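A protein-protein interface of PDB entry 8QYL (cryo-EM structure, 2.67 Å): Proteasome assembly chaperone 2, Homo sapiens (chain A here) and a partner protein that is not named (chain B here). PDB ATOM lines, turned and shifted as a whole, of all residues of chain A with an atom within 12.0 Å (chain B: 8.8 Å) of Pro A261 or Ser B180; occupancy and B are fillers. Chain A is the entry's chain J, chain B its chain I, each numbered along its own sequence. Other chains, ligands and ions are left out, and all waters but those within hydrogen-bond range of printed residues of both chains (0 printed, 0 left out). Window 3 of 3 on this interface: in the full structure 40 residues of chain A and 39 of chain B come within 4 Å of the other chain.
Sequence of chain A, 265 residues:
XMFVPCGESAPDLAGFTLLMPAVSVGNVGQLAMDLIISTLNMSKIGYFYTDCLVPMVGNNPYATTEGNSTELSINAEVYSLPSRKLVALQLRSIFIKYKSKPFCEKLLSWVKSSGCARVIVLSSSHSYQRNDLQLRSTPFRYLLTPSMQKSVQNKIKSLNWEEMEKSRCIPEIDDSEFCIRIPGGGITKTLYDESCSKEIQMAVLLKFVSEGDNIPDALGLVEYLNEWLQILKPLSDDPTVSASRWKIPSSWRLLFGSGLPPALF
O of Tyr B175 is in hydrogen-bond range of OG of Ser A258, at 3.3 Å. The backbone NH of Gly A259 sits at hydrogen-bond distance from the backbone carbonyl oxygen of Glu B179 (3.3 Å).
O of Glu B179 lies within hydrogen-bond range of OG1 of Thr B177 (3.0 Å). The backbone NH of Gly B182 lies close to the side-chain hydroxyl of Ser B180. The backbone carbonyl oxygen (O) of Ser B180 is in hydrogen-bond range of the side-chain hydroxyl (OG) of Ser B183, at 2.7 Å.
Leu A254 touches Thr B177 (CD2 to O, 3.6 Å). Lys B176 touches Ser A258 (CA to OG, 3.7 Å). Ser A258 touches Thr B177 (CA to O, 3.4 Å). Thr B177 touches Gly A259. Gly A259 touches Ser B178 (CA to O, 3.7 Å). CB of Ser B180 touches O of Leu A260, 3.9 Å away. Ser B180 touches Pro A261.
Of the printed residues of chain B, Leu A254 touches Thr B177. Printed residues of chain B within 4 Å of Ser A258: Tyr B175, Lys B176 and Thr B177. Pro A261 touches one residue of chain B. Val B172 touches none of the printed residues of chain A. Printed residues of chain A within 4 Å of Tyr B175: Ser A258. Printed residues of chain A within 4 Å of Lys B176: Ser A258. Ser B178 touches just one residue of chain A: Gly A259. No residue of chain A comes within 4 Å of Thr B181. No residue of chain A comes within 4 Å of Gly B182. Pro B185 touches none of the printed residues of chain A. The nearest residue of chain B that does not touch Pro A261 is Thr B181 (6.6 Å).
Of the 12 printed residues of chain B, 6 touch a printed residue of chain A. Of the 12 printed residues of chain A, 5 touch a printed residue of chain B. Printed residues of chain A that touch a printed residue of chain B: Leu A254, Ser A258, Gly A259, Leu A260 and Pro A261. Hydrophobic or aromatic side chains of chain A that line the printed part of chain B: Leu A254. Among the printed residues, 9 pairs touch across the chains. Among the printed residues, no Asp or Glu carboxylate lies within 4 Å of a Lys or Arg side-chain nitrogen of the other chain.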
ATOM      1  N   ARG A 253     -16.633 -32.120   3.833  1.00  0.00           N
ATOM      2  CA  ARG A 253     -17.510 -31.026   4.213  1.00  0.00           C
ATOM      3  C   ARG A 253     -17.772 -31.110   5.708  1.00  0.00           C
ATOM      4  O   ARG A 253     -17.650 -32.174   6.318  1.00  0.00           O
ATOM      5  CB  ARG A 253     -18.832 -31.063   3.438  1.00  0.00           C
ATOM      6  CG  ARG A 253     -19.628 -32.333   3.645  1.00  0.00           C
ATOM      7  CD  ARG A 253     -20.905 -32.329   2.826  1.00  0.00           C
ATOM      8  NE  ARG A 253     -21.888 -31.389   3.350  1.00  0.00           N
ATOM      9  CZ  ARG A 253     -23.060 -31.738   3.861  1.00  0.00           C
ATOM     10  NH1 ARG A 253     -23.430 -33.005   3.937  1.00  0.00           N
ATOM     11  NH2 ARG A 253     -23.879 -30.793   4.311  1.00  0.00           N
ATOM     12  N   LEU A 254     -18.126 -29.966   6.293  1.00  0.00           N
ATOM     13  CA  LEU A 254     -18.390 -29.865   7.729  1.00  0.00           C
ATOM     14  C   LEU A 254     -17.202 -30.362   8.548  1.00  0.00           C
ATOM     15  O   LEU A 254     -17.361 -31.079   9.536  1.00  0.00           O
ATOM     16  CB  LEU A 254     -19.664 -30.620   8.114  1.00  0.00           C
ATOM     17  CG  LEU A 254     -20.925 -30.281   7.324  1.00  0.00           C
ATOM     18  CD1 LEU A 254     -21.963 -31.362   7.516  1.00  0.00           C
ATOM     19  CD2 LEU A 254     -21.466 -28.936   7.750  1.00  0.00           C
ATOM     20  N   PHE A 256     -15.380 -28.671  10.454  1.00  0.00           N
ATOM     21  CA  PHE A 256     -15.289 -27.952  11.714  1.00  0.00           C
ATOM     22  C   PHE A 256     -16.511 -28.147  12.598  1.00  0.00           C
ATOM     23  O   PHE A 256     -16.537 -27.625  13.716  1.00  0.00           O
ATOM     24  CB  PHE A 256     -15.079 -26.457  11.453  1.00  0.00           C
ATOM     25  CG  PHE A 256     -13.638 -26.047  11.383  1.00  0.00           C
ATOM     26  CD1 PHE A 256     -12.900 -25.863  12.537  1.00  0.00           C
ATOM     27  CD2 PHE A 256     -13.024 -25.835  10.164  1.00  0.00           C
ATOM     28  CE1 PHE A 256     -11.578 -25.483  12.477  1.00  0.00           C
ATOM     29  CE2 PHE A 256     -11.702 -25.453  10.099  1.00  0.00           C
ATOM     30  CZ  PHE A 256     -10.979 -25.277  11.257  1.00  0.00           C
ATOM     31  N   GLY A 257     -17.525 -28.871  12.132  1.00  0.00           N
ATOM     32  CA  GLY A 257     -18.698 -29.128  12.941  1.00  0.00           C
ATOM     33  C   GLY A 257     -19.995 -28.679  12.303  1.00  0.00           C
ATOM     34  O   GLY A 257     -20.063 -28.483  11.087  1.00  0.00           O
ATOM     35  N   SER A 258     -21.032 -28.508  13.118  1.00  0.00           N
ATOM     36  CA  SER A 258     -22.344 -28.101  12.637  1.00  0.00           C
ATOM     37  C   SER A 258     -22.398 -26.582  12.499  1.00  0.00           C
ATOM     38  O   SER A 258     -21.382 -25.887  12.576  1.00  0.00           O
ATOM     39  CB  SER A 258     -23.433 -28.622  13.570  1.00  0.00           C
ATOM     40  OG  SER A 258     -23.358 -30.026  13.711  1.00  0.00           O
ATOM     41  N   GLY A 259     -23.599 -26.047  12.298  1.00  0.00           N
ATOM     42  CA  GLY A 259     -23.778 -24.627  12.098  1.00  0.00           C
ATOM     43  C   GLY A 259     -23.686 -23.828  13.383  1.00  0.00           C
ATOM     44  O   GLY A 259     -23.474 -24.352  14.476  1.00  0.00           O
ATOM     45  N   LEU A 260     -23.854 -22.529  13.233  1.00  0.00           N
ATOM     46  CA  LEU A 260     -23.715 -21.532  14.290  1.00  0.00           C
ATOM     47  C   LEU A 260     -25.067 -21.257  14.940  1.00  0.00           C
ATOM     48  O   LEU A 260     -26.036 -20.961  14.233  1.00  0.00           O
ATOM     49  CB  LEU A 260     -23.141 -20.244  13.720  1.00  0.00           C
ATOM     50  CG  LEU A 260     -22.837 -19.075  14.650  1.00  0.00           C
ATOM     51  CD1 LEU A 260     -21.848 -19.473  15.722  1.00  0.00           C
ATOM     52  CD2 LEU A 260     -22.305 -17.916  13.834  1.00  0.00           C
ATOM     53  N   PRO A 261     -25.175 -21.355  16.268  1.00  0.00           N
ATOM     54  CA  PRO A 261     -26.459 -21.092  16.916  1.00  0.00           C
ATOM     55  C   PRO A 261     -26.849 -19.631  16.782  1.00  0.00           C
ATOM     56  O   PRO A 261     -25.982 -18.749  16.662  1.00  0.00           O
ATOM     57  CB  PRO A 261     -26.200 -21.470  18.385  1.00  0.00           C
ATOM     58  CG  PRO A 261     -24.729 -21.398  18.545  1.00  0.00           C
ATOM     59  CD  PRO A 261     -24.152 -21.801  17.227  1.00  0.00           C
ATOM     60  N   PRO A 262     -28.149 -19.325  16.798  1.00  0.00           N
ATOM     61  CA  PRO A 262     -28.583 -17.932  16.631  1.00  0.00           C
ATOM     62  C   PRO A 262     -28.592 -17.147  17.933  1.00  0.00           C
ATOM     63  O   PRO A 262     -28.304 -17.696  19.000  1.00  0.00           O
ATOM     64  CB  PRO A 262     -29.996 -18.083  16.061  1.00  0.00           C
ATOM     65  CG  PRO A 262     -30.490 -19.356  16.658  1.00  0.00           C
ATOM     66  CD  PRO A 262     -29.292 -20.249  16.889  1.00  0.00           C
ATOM     67  N   ALA A 263     -28.928 -15.858  17.844  1.00  0.00           N
ATOM     68  CA  ALA A 263     -28.974 -14.957  18.998  1.00  0.00           C
ATOM     69  C   ALA A 263     -27.618 -14.858  19.690  1.00  0.00           C
ATOM     70  O   ALA A 263     -27.529 -14.797  20.917  1.00  0.00           O
ATOM     71  CB  ALA A 263     -30.060 -15.379  19.991  1.00  0.00           C
ATOM     72  N   LEU A 264     -26.557 -14.846  18.903  1.00  0.00           N
ATOM     73  CA  LEU A 264     -25.207 -14.697  19.437  1.00  0.00           C
ATOM     74  C   LEU A 264     -24.418 -13.590  18.759  1.00  0.00           C
ATOM     75  O   LEU A 264     -23.663 -12.885  19.431  1.00  0.00           O
ATOM     76  CB  LEU A 264     -24.449 -16.025  19.310  1.00  0.00           C
ATOM     77  CG  LEU A 264     -23.471 -16.357  20.432  1.00  0.00           C
ATOM     78  CD1 LEU A 264     -24.196 -16.367  21.754  1.00  0.00           C
ATOM     79  CD2 LEU A 264     -22.809 -17.692  20.178  1.00  0.00           C
ATOM     80  N   PHE A 265     -24.576 -13.414  17.452  1.00  0.00           N
ATOM     81  CA  PHE A 265     -23.820 -12.412  16.714  1.00  0.00           C
ATOM     82  C   PHE A 265     -24.737 -11.320  16.183  1.00  0.00           C
ATOM     83  O   PHE A 265     -25.785 -11.602  15.606  1.00  0.00           O
ATOM     84  CB  PHE A 265     -23.053 -13.059  15.560  1.00  0.00           C
ATOM     85  CG  PHE A 265     -21.864 -13.861  15.996  1.00  0.00           C
ATOM     86  CD1 PHE A 265     -20.638 -13.256  16.185  1.00  0.00           C
ATOM     87  CD2 PHE A 265     -21.974 -15.218  16.219  1.00  0.00           C
ATOM     88  CE1 PHE A 265     -19.547 -13.989  16.590  1.00  0.00           C
ATOM     89  CE2 PHE A 265     -20.886 -15.956  16.622  1.00  0.00           C
ATOM     90  CZ  PHE A 265     -19.671 -15.340  16.808  1.00  0.00           C
ATOM     91  N   VAL B 172     -28.156 -36.071  20.182  1.00  0.00           N
ATOM     92  CA  VAL B 172     -28.412 -35.316  18.962  1.00  0.00           C
ATOM     93  C   VAL B 172     -27.251 -34.394  18.603  1.00  0.00           C
ATOM     94  O   VAL B 172     -27.100 -34.031  17.433  1.00  0.00           O
ATOM     95  CB  VAL B 172     -29.730 -34.527  19.095  1.00  0.00           C
ATOM     96  CG1 VAL B 172     -29.566 -33.355  20.042  1.00  0.00           C
ATOM     97  CG2 VAL B 172     -30.224 -34.070  17.735  1.00  0.00           C
ATOM     98  N   TYR B 175     -24.879 -35.477  15.683  1.00  0.00           N
ATOM     99  CA  TYR B 175     -25.274 -35.361  14.288  1.00  0.00           C
ATOM    100  C   TYR B 175     -24.692 -34.094  13.674  1.00  0.00           C
ATOM    101  O   TYR B 175     -24.678 -33.034  14.303  1.00  0.00           O
ATOM    102  CB  TYR B 175     -26.797 -35.351  14.179  1.00  0.00           C
ATOM    103  CG  TYR B 175     -27.337 -35.760  12.833  1.00  0.00           C
ATOM    104  CD1 TYR B 175     -27.238 -37.068  12.393  1.00  0.00           C
ATOM    105  CD2 TYR B 175     -27.960 -34.840  12.009  1.00  0.00           C
ATOM    106  CE1 TYR B 175     -27.736 -37.445  11.165  1.00  0.00           C
ATOM    107  CE2 TYR B 175     -28.461 -35.207  10.782  1.00  0.00           C
ATOM    108  CZ  TYR B 175     -28.346 -36.510  10.364  1.00  0.00           C
ATOM    109  OH  TYR B 175     -28.845 -36.876   9.138  1.00  0.00           O
ATOM    110  N   LYS B 176     -24.215 -34.208  12.438  1.00  0.00           N
ATOM    111  CA  LYS B 176     -23.583 -33.102  11.729  1.00  0.00           C
ATOM    112  C   LYS B 176     -24.514 -32.607  10.632  1.00  0.00           C
ATOM    113  O   LYS B 176     -24.906 -33.377   9.750  1.00  0.00           O
ATOM    114  CB  LYS B 176     -22.240 -33.530  11.141  1.00  0.00           C
ATOM    115  CG  LYS B 176     -21.159 -33.737  12.178  1.00  0.00           C
ATOM    116  CD  LYS B 176     -19.994 -34.506  11.604  1.00  0.00           C
ATOM    117  CE  LYS B 176     -18.818 -34.488  12.556  1.00  0.00           C
ATOM    118  NZ  LYS B 176     -17.647 -35.210  11.993  1.00  0.00           N
ATOM    119  N   THR B 177     -24.852 -31.322  10.684  1.00  0.00           N
ATOM    120  CA  THR B 177     -25.734 -30.691   9.714  1.00  0.00           C
ATOM    121  C   THR B 177     -25.161 -29.345   9.302  1.00  0.00           C
ATOM    122  O   THR B 177     -24.320 -28.765   9.991  1.00  0.00           O
ATOM    123  CB  THR B 177     -27.150 -30.488  10.270  1.00  0.00           C
ATOM    124  OG1 THR B 177     -27.076 -29.901  11.576  1.00  0.00           O
ATOM    125  CG2 THR B 177     -27.891 -31.799  10.346  1.00  0.00           C
ATOM    126  N   SER B 178     -25.634 -28.853   8.157  1.00  0.00           N
ATOM    127  CA  SER B 178     -25.239 -27.523   7.713  1.00  0.00           C
ATOM    128  C   SER B 178     -25.856 -26.435   8.581  1.00  0.00           C
ATOM    129  O   SER B 178     -25.248 -25.376   8.767  1.00  0.00           O
ATOM    130  CB  SER B 178     -25.628 -27.323   6.251  1.00  0.00           C
ATOM    131  OG  SER B 178     -25.064 -26.133   5.736  1.00  0.00           O
ATOM    132  N   GLU B 179     -27.050 -26.672   9.117  1.00  0.00           N
ATOM    133  CA  GLU B 179     -27.716 -25.707   9.975  1.00  0.00           C
ATOM    134  C   GLU B 179     -27.432 -26.013  11.445  1.00  0.00           C
ATOM    135  O   GLU B 179     -26.741 -26.974  11.786  1.00  0.00           O
ATOM    136  CB  GLU B 179     -29.218 -25.690   9.698  1.00  0.00           C
ATOM    137  CG  GLU B 179     -29.949 -26.945  10.131  1.00  0.00           C
ATOM    138  CD  GLU B 179     -29.900 -28.038   9.083  1.00  0.00           C
ATOM    139  OE1 GLU B 179     -29.064 -27.946   8.161  1.00  0.00           O
ATOM    140  OE2 GLU B 179     -30.699 -28.993   9.182  1.00  0.00           O
ATOM    141  N   SER B 180     -27.970 -25.176  12.327  1.00  0.00           N
ATOM    142  CA  SER B 180     -27.756 -25.351  13.756  1.00  0.00           C
ATOM    143  C   SER B 180     -28.414 -26.634  14.245  1.00  0.00           C
ATOM    144  O   SER B 180     -29.555 -26.942  13.890  1.00  0.00           O
ATOM    145  CB  SER B 180     -28.311 -24.153  14.525  1.00  0.00           C
ATOM    146  OG  SER B 180     -28.232 -24.363  15.921  1.00  0.00           O
ATOM    147  N   THR B 181     -27.684 -27.385  15.072  1.00  0.00           N
ATOM    148  CA  THR B 181     -28.172 -28.665  15.570  1.00  0.00           C
ATOM    149  C   THR B 181     -29.297 -28.518  16.586  1.00  0.00           C
ATOM    150  O   THR B 181     -29.957 -29.514  16.897  1.00  0.00           O
ATOM    151  CB  THR B 181     -27.020 -29.465  16.187  1.00  0.00           C
ATOM    152  OG1 THR B 181     -27.451 -30.803  16.455  1.00  0.00           O
ATOM    153  CG2 THR B 181     -26.552 -28.821  17.483  1.00  0.00           C
ATOM    154  N   GLY B 182     -29.532 -27.317  17.106  1.00  0.00           N
ATOM    155  CA  GLY B 182     -30.609 -27.082  18.043  1.00  0.00           C
ATOM    156  C   GLY B 182     -31.960 -26.821  17.425  1.00  0.00           C
ATOM    157  O   GLY B 182     -32.932 -26.599  18.152  1.00  0.00           O
ATOM    158  N   SER B 183     -32.054 -26.840  16.097  1.00  0.00           N
ATOM    159  CA  SER B 183     -33.309 -26.607  15.398  1.00  0.00           C
ATOM    160  C   SER B 183     -33.923 -27.878  14.826  1.00  0.00           C
ATOM    161  O   SER B 183     -35.052 -27.829  14.328  1.00  0.00           O
ATOM    162  CB  SER B 183     -33.101 -25.594  14.266  1.00  0.00           C
ATOM    163  OG  SER B 183     -32.010 -25.969  13.443  1.00  0.00           O
ATOM    164  N   LEU B 184     -33.217 -29.001  14.885  1.00  0.00           N
ATOM    165  CA  LEU B 184     -33.742 -30.234  14.319  1.00  0.00           C
ATOM    166  C   LEU B 184     -34.872 -30.777  15.191  1.00  0.00           C
ATOM    167  O   LEU B 184     -34.813 -30.679  16.420  1.00  0.00           O
ATOM    168  CB  LEU B 184     -32.634 -31.277  14.195  1.00  0.00           C
ATOM    169  CG  LEU B 184     -31.346 -30.827  13.508  1.00  0.00           C
ATOM    170  CD1 LEU B 184     -30.279 -31.895  13.632  1.00  0.00           C
ATOM    171  CD2 LEU B 184     -31.607 -30.501  12.051  1.00  0.00           C
ATOM    172  N   PRO B 185     -35.913 -31.351  14.590  1.00  0.00           N
ATOM    173  CA  PRO B 185     -36.984 -31.981  15.374  1.00  0.00           C
ATOM    174  C   PRO B 185     -36.547 -33.341  15.894  1.00  0.00           C
ATOM    175  O   PRO B 185     -36.440 -34.310  15.137  1.00  0.00           O
ATOM    176  CB  PRO B 185     -38.131 -32.095  14.360  1.00  0.00           C
ATOM    177  CG  PRO B 185     -37.456 -32.165  13.038  1.00  0.00           C
ATOM    178  CD  PRO B 185     -36.211 -31.333  13.147  1.00  0.00           C
